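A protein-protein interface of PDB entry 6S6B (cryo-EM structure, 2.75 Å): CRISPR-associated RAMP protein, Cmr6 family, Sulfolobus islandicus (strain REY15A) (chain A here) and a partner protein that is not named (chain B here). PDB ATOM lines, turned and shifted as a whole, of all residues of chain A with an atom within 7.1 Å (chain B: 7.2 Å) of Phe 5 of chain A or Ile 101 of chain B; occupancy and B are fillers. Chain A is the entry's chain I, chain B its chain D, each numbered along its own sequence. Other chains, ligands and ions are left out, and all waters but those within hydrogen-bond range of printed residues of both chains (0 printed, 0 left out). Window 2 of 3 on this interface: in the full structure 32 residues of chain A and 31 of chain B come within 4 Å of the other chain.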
ATOM      1  N   ALA A   2     -23.958  34.135 -21.800  1.00  0.00           N
ATOM      2  CA  ALA A   2     -24.212  35.507 -21.376  1.00  0.00           C
ATOM      3  C   ALA A   2     -24.149  35.620 -19.862  1.00  0.00           C
ATOM      4  O   ALA A   2     -24.263  34.626 -19.153  1.00  0.00           O
ATOM      5  CB  ALA A   2     -25.565  35.981 -21.886  1.00  0.00           C
ATOM      6  N   ILE A   3     -23.962  36.843 -19.366  1.00  0.00           N
ATOM      7  CA  ILE A   3     -23.982  37.048 -17.925  1.00  0.00           C
ATOM      8  C   ILE A   3     -25.366  36.756 -17.366  1.00  0.00           C
ATOM      9  O   ILE A   3     -25.501  36.315 -16.220  1.00  0.00           O
ATOM     10  CB  ILE A   3     -23.519  38.473 -17.586  1.00  0.00           C
ATOM     11  CG1 ILE A   3     -23.500  38.685 -16.076  1.00  0.00           C
ATOM     12  CG2 ILE A   3     -24.406  39.502 -18.274  1.00  0.00           C
ATOM     13  CD1 ILE A   3     -22.971  40.027 -15.671  1.00  0.00           C
ATOM     14  N   ASP A   4     -26.414  36.975 -18.161  1.00  0.00           N
ATOM     15  CA  ASP A   4     -27.752  36.556 -17.769  1.00  0.00           C
ATOM     16  C   ASP A   4     -27.884  35.043 -17.703  1.00  0.00           C
ATOM     17  O   ASP A   4     -28.865  34.544 -17.145  1.00  0.00           O
ATOM     18  CB  ASP A   4     -28.787  37.119 -18.743  1.00  0.00           C
ATOM     19  CG  ASP A   4     -28.574  38.591 -19.037  1.00  0.00           C
ATOM     20  OD1 ASP A   4     -28.646  39.406 -18.096  1.00  0.00           O
ATOM     21  OD2 ASP A   4     -28.333  38.931 -20.214  1.00  0.00           O
ATOM     22  N   PHE A   5     -26.928  34.309 -18.262  1.00  0.00           N
ATOM     23  CA  PHE A   5     -26.954  32.857 -18.244  1.00  0.00           C
ATOM     24  C   PHE A   5     -26.250  32.289 -17.025  1.00  0.00           C
ATOM     25  O   PHE A   5     -26.640  31.226 -16.531  1.00  0.00           O
ATOM     26  CB  PHE A   5     -26.285  32.310 -19.507  1.00  0.00           C
ATOM     27  CG  PHE A   5     -26.461  30.839 -19.702  1.00  0.00           C
ATOM     28  CD1 PHE A   5     -27.551  30.342 -20.390  1.00  0.00           C
ATOM     29  CD2 PHE A   5     -25.557  29.949 -19.163  1.00  0.00           C
ATOM     30  CE1 PHE A   5     -27.711  28.992 -20.572  1.00  0.00           C
ATOM     31  CE2 PHE A   5     -25.718  28.594 -19.334  1.00  0.00           C
ATOM     32  CZ  PHE A   5     -26.798  28.115 -20.039  1.00  0.00           C
ATOM     33  N   LEU A   6     -25.210  32.969 -16.542  1.00  0.00           N
ATOM     34  CA  LEU A   6     -24.431  32.456 -15.422  1.00  0.00           C
ATOM     35  C   LEU A   6     -25.147  32.680 -14.100  1.00  0.00           C
ATOM     36  O   LEU A   6     -25.150  31.799 -13.236  1.00  0.00           O
ATOM     37  CB  LEU A   6     -23.056  33.116 -15.392  1.00  0.00           C
ATOM     38  CG  LEU A   6     -22.113  32.737 -16.527  1.00  0.00           C
ATOM     39  CD1 LEU A   6     -20.912  33.652 -16.539  1.00  0.00           C
ATOM     40  CD2 LEU A   6     -21.685  31.301 -16.379  1.00  0.00           C
ATOM     41  N   VAL A   7     -25.755  33.854 -13.927  1.00  0.00           N
ATOM     42  CA  VAL A   7     -26.504  34.141 -12.713  1.00  0.00           C
ATOM     43  C   VAL A   7     -27.614  33.132 -12.477  1.00  0.00           C
ATOM     44  O   VAL A   7     -28.085  32.985 -11.346  1.00  0.00           O
ATOM     45  CB  VAL A   7     -27.066  35.572 -12.776  1.00  0.00           C
ATOM     46  CG1 VAL A   7     -25.951  36.556 -13.037  1.00  0.00           C
ATOM     47  CG2 VAL A   7     -28.105  35.673 -13.867  1.00  0.00           C
ATOM     48  N   ASN A   8     -28.045  32.426 -13.517  1.00  0.00           N
ATOM     49  CA  ASN A   8     -29.084  31.418 -13.399  1.00  0.00           C
ATOM     50  C   ASN A   8     -28.532  30.005 -13.342  1.00  0.00           C
ATOM     51  O   ASN A   8     -29.314  29.053 -13.333  1.00  0.00           O
ATOM     52  CB  ASN A   8     -30.064  31.531 -14.570  1.00  0.00           C
ATOM     53  CG  ASN A   8     -30.612  32.935 -14.742  1.00  0.00           C
ATOM     54  OD1 ASN A   8     -30.974  33.341 -15.844  1.00  0.00           O
ATOM     55  ND2 ASN A   8     -30.685  33.679 -13.646  1.00  0.00           N
ATOM     56  N   ILE A   9     -27.208  29.842 -13.300  1.00  0.00           N
ATOM     57  CA  ILE A   9     -26.640  28.504 -13.424  1.00  0.00           C
ATOM     58  C   ILE A   9     -26.853  27.696 -12.152  1.00  0.00           C
ATOM     59  O   ILE A   9     -26.940  26.464 -12.203  1.00  0.00           O
ATOM     60  CB  ILE A   9     -25.148  28.584 -13.798  1.00  0.00           C
ATOM     61  CG1 ILE A   9     -24.711  27.293 -14.482  1.00  0.00           C
ATOM     62  CG2 ILE A   9     -24.284  28.838 -12.577  1.00  0.00           C
ATOM     63  CD1 ILE A   9     -25.108  27.232 -15.925  1.00  0.00           C
ATOM     64  N   LEU A  10     -26.950  28.359 -11.000  1.00  0.00           N
ATOM     65  CA  LEU A  10     -27.091  27.625  -9.749  1.00  0.00           C
ATOM     66  C   LEU A  10     -28.497  27.070  -9.592  1.00  0.00           C
ATOM     67  O   LEU A  10     -28.682  25.981  -9.038  1.00  0.00           O
ATOM     68  CB  LEU A  10     -26.730  28.525  -8.573  1.00  0.00           C
ATOM     69  CG  LEU A  10     -25.286  28.419  -8.092  1.00  0.00           C
ATOM     70  CD1 LEU A  10     -25.135  29.091  -6.751  1.00  0.00           C
ATOM     71  CD2 LEU A  10     -24.856  26.969  -8.009  1.00  0.00           C
ATOM     72  N   LEU A  12     -30.170  25.992 -12.031  1.00  0.00           N
ATOM     73  CA  LEU A  12     -30.231  24.846 -12.928  1.00  0.00           C
ATOM     74  C   LEU A  12     -29.786  23.569 -12.238  1.00  0.00           C
ATOM     75  O   LEU A  12     -30.260  22.482 -12.583  1.00  0.00           O
ATOM     76  CB  LEU A  12     -29.370  25.094 -14.160  1.00  0.00           C
ATOM     77  CG  LEU A  12     -29.730  26.311 -14.999  1.00  0.00           C
ATOM     78  CD1 LEU A  12     -29.005  26.230 -16.317  1.00  0.00           C
ATOM     79  CD2 LEU A  12     -31.228  26.389 -15.207  1.00  0.00           C
ATOM     80  N   GLU A  15     -32.642  22.015  -9.971  1.00  0.00           N
ATOM     81  CA  GLU A  15     -33.880  21.663 -10.651  1.00  0.00           C
ATOM     82  C   GLU A  15     -33.739  20.471 -11.587  1.00  0.00           C
ATOM     83  O   GLU A  15     -34.737  20.041 -12.170  1.00  0.00           O
ATOM     84  CB  GLU A  15     -34.414  22.869 -11.428  1.00  0.00           C
ATOM     85  CG  GLU A  15     -33.778  23.072 -12.783  1.00  0.00           C
ATOM     86  CD  GLU A  15     -34.472  24.154 -13.583  1.00  0.00           C
ATOM     87  OE1 GLU A  15     -35.379  24.809 -13.029  1.00  0.00           O
ATOM     88  OE2 GLU A  15     -34.113  24.351 -14.762  1.00  0.00           O
ATOM     89  N   LEU A  28     -18.843  26.655 -15.001  1.00  0.00           N
ATOM     90  CA  LEU A  28     -19.517  27.941 -15.111  1.00  0.00           C
ATOM     91  C   LEU A  28     -19.730  28.568 -13.743  1.00  0.00           C
ATOM     92  O   LEU A  28     -19.610  29.788 -13.588  1.00  0.00           O
ATOM     93  CB  LEU A  28     -20.847  27.777 -15.839  1.00  0.00           C
ATOM     94  CG  LEU A  28     -20.712  27.425 -17.318  1.00  0.00           C
ATOM     95  CD1 LEU A  28     -22.060  27.417 -17.982  1.00  0.00           C
ATOM     96  CD2 LEU A  28     -19.788  28.395 -18.005  1.00  0.00           C
ATOM     97  N   ILE B  98     -22.933  20.141 -23.148  1.00  0.00           N
ATOM     98  CA  ILE B  98     -23.799  21.286 -23.379  1.00  0.00           C
ATOM     99  C   ILE B  98     -24.461  21.689 -22.074  1.00  0.00           C
ATOM    100  O   ILE B  98     -24.760  20.842 -21.225  1.00  0.00           O
ATOM    101  CB  ILE B  98     -24.858  20.970 -24.453  1.00  0.00           C
ATOM    102  CG1 ILE B  98     -25.651  22.216 -24.817  1.00  0.00           C
ATOM    103  CG2 ILE B  98     -25.787  19.880 -23.985  1.00  0.00           C
ATOM    104  CD1 ILE B  98     -26.574  22.002 -25.962  1.00  0.00           C
ATOM    105  N   ILE B  99     -24.671  22.987 -21.904  1.00  0.00           N
ATOM    106  CA  ILE B  99     -25.466  23.529 -20.815  1.00  0.00           C
ATOM    107  C   ILE B  99     -26.406  24.560 -21.414  1.00  0.00           C
ATOM    108  O   ILE B  99     -25.967  25.460 -22.134  1.00  0.00           O
ATOM    109  CB  ILE B  99     -24.593  24.147 -19.705  1.00  0.00           C
ATOM    110  CG1 ILE B  99     -25.459  24.849 -18.667  1.00  0.00           C
ATOM    111  CG2 ILE B  99     -23.578  25.102 -20.278  1.00  0.00           C
ATOM    112  CD1 ILE B  99     -26.304  23.910 -17.851  1.00  0.00           C
ATOM    113  N   GLU B 100     -27.697  24.415 -21.144  1.00  0.00           N
ATOM    114  CA  GLU B 100     -28.676  25.285 -21.769  1.00  0.00           C
ATOM    115  C   GLU B 100     -29.880  25.425 -20.857  1.00  0.00           C
ATOM    116  O   GLU B 100     -30.138  24.582 -19.996  1.00  0.00           O
ATOM    117  CB  GLU B 100     -29.099  24.744 -23.136  1.00  0.00           C
ATOM    118  CG  GLU B 100     -30.268  23.780 -23.087  1.00  0.00           C
ATOM    119  CD  GLU B 100     -29.877  22.382 -22.652  1.00  0.00           C
ATOM    120  OE1 GLU B 100     -28.897  22.232 -21.896  1.00  0.00           O
ATOM    121  OE2 GLU B 100     -30.560  21.424 -23.068  1.00  0.00           O
ATOM    122  N   ILE B 101     -30.616  26.514 -21.058  1.00  0.00           N
ATOM    123  CA  ILE B 101     -31.860  26.759 -20.338  1.00  0.00           C
ATOM    124  C   ILE B 101     -32.962  26.699 -21.386  1.00  0.00           C
ATOM    125  O   ILE B 101     -32.682  26.489 -22.572  1.00  0.00           O
ATOM    126  CB  ILE B 101     -31.824  28.111 -19.601  1.00  0.00           C
ATOM    127  CG1 ILE B 101     -30.560  28.214 -18.757  1.00  0.00           C
ATOM    128  CG2 ILE B 101     -32.987  28.244 -18.635  1.00  0.00           C
ATOM    129  CD1 ILE B 101     -30.326  29.592 -18.190  1.00  0.00           C
ATOM    130  N   ASP B 102     -34.217  26.848 -20.966  1.00  0.00           N
ATOM    131  CA  ASP B 102     -35.352  26.952 -21.880  1.00  0.00           C
ATOM    132  C   ASP B 102     -35.491  25.686 -22.726  1.00  0.00           C
ATOM    133  O   ASP B 102     -35.351  25.703 -23.951  1.00  0.00           O
ATOM    134  CB  ASP B 102     -35.218  28.190 -22.773  1.00  0.00           C
ATOM    135  CG  ASP B 102     -34.725  29.403 -22.019  1.00  0.00           C
ATOM    136  OD1 ASP B 102     -35.202  29.637 -20.888  1.00  0.00           O
ATOM    137  OD2 ASP B 102     -33.853  30.120 -22.558  1.00  0.00           O
ATOM    138  N   SER B 103     -35.759  24.578 -22.043  1.00  0.00           N
ATOM    139  CA  SER B 103     -35.971  23.312 -22.730  1.00  0.00           C
ATOM    140  C   SER B 103     -36.745  22.377 -21.817  1.00  0.00           C
ATOM    141  O   SER B 103     -36.306  22.096 -20.697  1.00  0.00           O
ATOM    142  CB  SER B 103     -34.640  22.676 -23.143  1.00  0.00           C
ATOM    143  OG  SER B 103     -34.060  23.375 -24.229  1.00  0.00           O
ATOM    144  N   ALA B 104     -37.896  21.903 -22.297  1.00  0.00           N
ATOM    145  CA  ALA B 104     -38.648  20.872 -21.593  1.00  0.00           C
ATOM    146  C   ALA B 104     -37.895  19.554 -21.511  1.00  0.00           C
ATOM    147  O   ALA B 104     -38.372  18.630 -20.843  1.00  0.00           O
ATOM    148  CB  ALA B 104     -39.998  20.646 -22.275  1.00  0.00           C
ATOM    149  N   ASP B 159     -35.237  21.342 -30.285  1.00  0.00           N
ATOM    150  CA  ASP B 159     -35.701  22.722 -30.312  1.00  0.00           C
ATOM    151  C   ASP B 159     -34.934  23.610 -29.339  1.00  0.00           C
ATOM    152  O   ASP B 159     -35.555  24.403 -28.625  1.00  0.00           O
ATOM    153  CB  ASP B 159     -37.191  22.796 -29.987  1.00  0.00           C
ATOM    154  CG  ASP B 159     -38.056  22.187 -31.070  1.00  0.00           C
ATOM    155  OD1 ASP B 159     -37.631  22.170 -32.244  1.00  0.00           O
ATOM    156  OD2 ASP B 159     -39.172  21.729 -30.746  1.00  0.00           O
ATOM    157  N   LEU B 160     -33.612  23.485 -29.267  1.00  0.00           N
ATOM    158  CA  LEU B 160     -32.828  24.409 -28.464  1.00  0.00           C
ATOM    159  C   LEU B 160     -32.782  25.775 -29.132  1.00  0.00           C
ATOM    160  O   LEU B 160     -32.741  25.884 -30.359  1.00  0.00           O
ATOM    161  CB  LEU B 160     -31.408  23.886 -28.265  1.00  0.00           C
ATOM    162  CG  LEU B 160     -31.197  22.391 -28.033  1.00  0.00           C
ATOM    163  CD1 LEU B 160     -29.719  22.069 -28.115  1.00  0.00           C
ATOM    164  CD2 LEU B 160     -31.758  21.966 -26.691  1.00  0.00           C
ATOM    165  N   LYS B 161     -32.789  26.823 -28.316  1.00  0.00           N
ATOM    166  CA  LYS B 161     -32.695  28.180 -28.837  1.00  0.00           C
ATOM    167  C   LYS B 161     -31.281  28.731 -28.749  1.00  0.00           C
ATOM    168  O   LYS B 161     -30.807  29.371 -29.692  1.00  0.00           O
ATOM    169  CB  LYS B 161     -33.657  29.098 -28.084  1.00  0.00           C
ATOM    170  CG  LYS B 161     -35.115  28.863 -28.419  1.00  0.00           C
ATOM    171  CD  LYS B 161     -35.373  29.076 -29.899  1.00  0.00           C
ATOM    172  CE  LYS B 161     -36.641  28.370 -30.344  1.00  0.00           C
ATOM    173  NZ  LYS B 161     -36.662  28.150 -31.814  1.00  0.00           N
ATOM    174  N   SER B 162     -30.602  28.494 -27.634  1.00  0.00           N
ATOM    175  CA  SER B 162     -29.228  28.933 -27.454  1.00  0.00           C
ATOM    176  C   SER B 162     -28.641  28.178 -26.274  1.00  0.00           C
ATOM    177  O   SER B 162     -29.340  27.885 -25.303  1.00  0.00           O
ATOM    178  CB  SER B 162     -29.136  30.442 -27.226  1.00  0.00           C
ATOM    179  OG  SER B 162     -29.435  30.777 -25.886  1.00  0.00           O
ATOM    180  N   ALA B 163     -27.354  27.862 -26.374  1.00  0.00           N
ATOM    181  CA  ALA B 163     -26.675  27.063 -25.369  1.00  0.00           C
ATOM    182  C   ALA B 163     -25.248  27.558 -25.214  1.00  0.00           C
ATOM    183  O   ALA B 163     -24.804  28.474 -25.909  1.00  0.00           O
ATOM    184  CB  ALA B 163     -26.694  25.582 -25.743  1.00  0.00           C
ATOM    185  N   ILE B 164     -24.527  26.942 -24.285  1.00  0.00           N
ATOM    186  CA  ILE B 164     -23.094  27.135 -24.124  1.00  0.00           C
ATOM    187  C   ILE B 164     -22.435  25.789 -24.335  1.00  0.00           C
ATOM    188  O   ILE B 164     -22.683  24.847 -23.575  1.00  0.00           O
ATOM    189  CB  ILE B 164     -22.734  27.702 -22.746  1.00  0.00           C
ATOM    190  CG1 ILE B 164     -23.437  29.033 -22.514  1.00  0.00           C
ATOM    191  CG2 ILE B 164     -21.241  27.873 -22.628  1.00  0.00           C
ATOM    192  CD1 ILE B 164     -22.923  29.762 -21.315  1.00  0.00           C
ATOM    193  N   TYR B 170     -20.853  30.406 -26.384  1.00  0.00           N
ATOM    194  CA  TYR B 170     -22.289  30.633 -26.396  1.00  0.00           C
ATOM    195  C   TYR B 170     -22.745  30.781 -27.838  1.00  0.00           C
ATOM    196  O   TYR B 170     -22.299  31.694 -28.540  1.00  0.00           O
ATOM    197  CB  TYR B 170     -22.654  31.878 -25.594  1.00  0.00           C
ATOM    198  CG  TYR B 170     -24.113  32.235 -25.699  1.00  0.00           C
ATOM    199  CD1 TYR B 170     -25.055  31.618 -24.893  1.00  0.00           C
ATOM    200  CD2 TYR B 170     -24.552  33.180 -26.610  1.00  0.00           C
ATOM    201  CE1 TYR B 170     -26.386  31.935 -24.987  1.00  0.00           C
ATOM    202  CE2 TYR B 170     -25.881  33.501 -26.712  1.00  0.00           C
ATOM    203  CZ  TYR B 170     -26.794  32.876 -25.899  1.00  0.00           C
ATOM    204  OH  TYR B 170     -28.128  33.194 -25.993  1.00  0.00           O
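O of Ile 99 of chain B sits at hydrogen-bond distance from N of Ile 164 of chain B, 3.0 Å away.
Among the printed residues, pairs that only touch across the chains: Phe 5 of chain A with Ile 164 of chain B (3.4 Å), Phe 5 of chain A with Ile 101 of chain B (3.5 Å), Phe 5 of chain A with Ile 99 of chain B (3.5 Å), Leu 12 of chain A with Ile 101 of chain B (3.5 Å), Leu 28 of chain A with Ile 99 of chain B (3.6 Å), Ile 9 of chain A with Ile 99 of chain B (3.6 Å), Phe 5 of chain A with Glu 100 of chain B (3.8 Å) and Leu 12 of chain A with Ile 99 of chain B (3.9 Å).
Phe 5 of chain A touches four residues of chain B.
Printed residues of chain B within 4 Å of Ile 9 of chain A: Ile 99 (3.6 Å).
Ile 101 of chain B touches just these residues of chain A: Phe 5 and Leu 12.
Ser 162 of chain B touches none of the printed residues of chain A.
Printed residues of chain A within 4 Å of Ile 164 of chain B: Phe 5.
The nearest printed residue of chain A that does not touch Glu 100 of chain B is Leu 12 of chain A (4.2 Å).
Of the 14 printed residues of chain B, 4 touch a printed residue of chain A.
Hydrophobic or aromatic side chains of chain B within 4 Å of the printed part of chain A: Ile 99, Ile 101 and Ile 164.
Hydrophobic or aromatic side chains of chain A within 4 Å of the printed part of chain B: Phe 5, Ile 9, Leu 12 and Leu 28.
Among the printed residues, 8 pairs touch across the chains.
Among the printed residues, no Asp or Glu carboxylate lies within 4 Å of a Lys or Arg side-chain nitrogen of the other chain.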
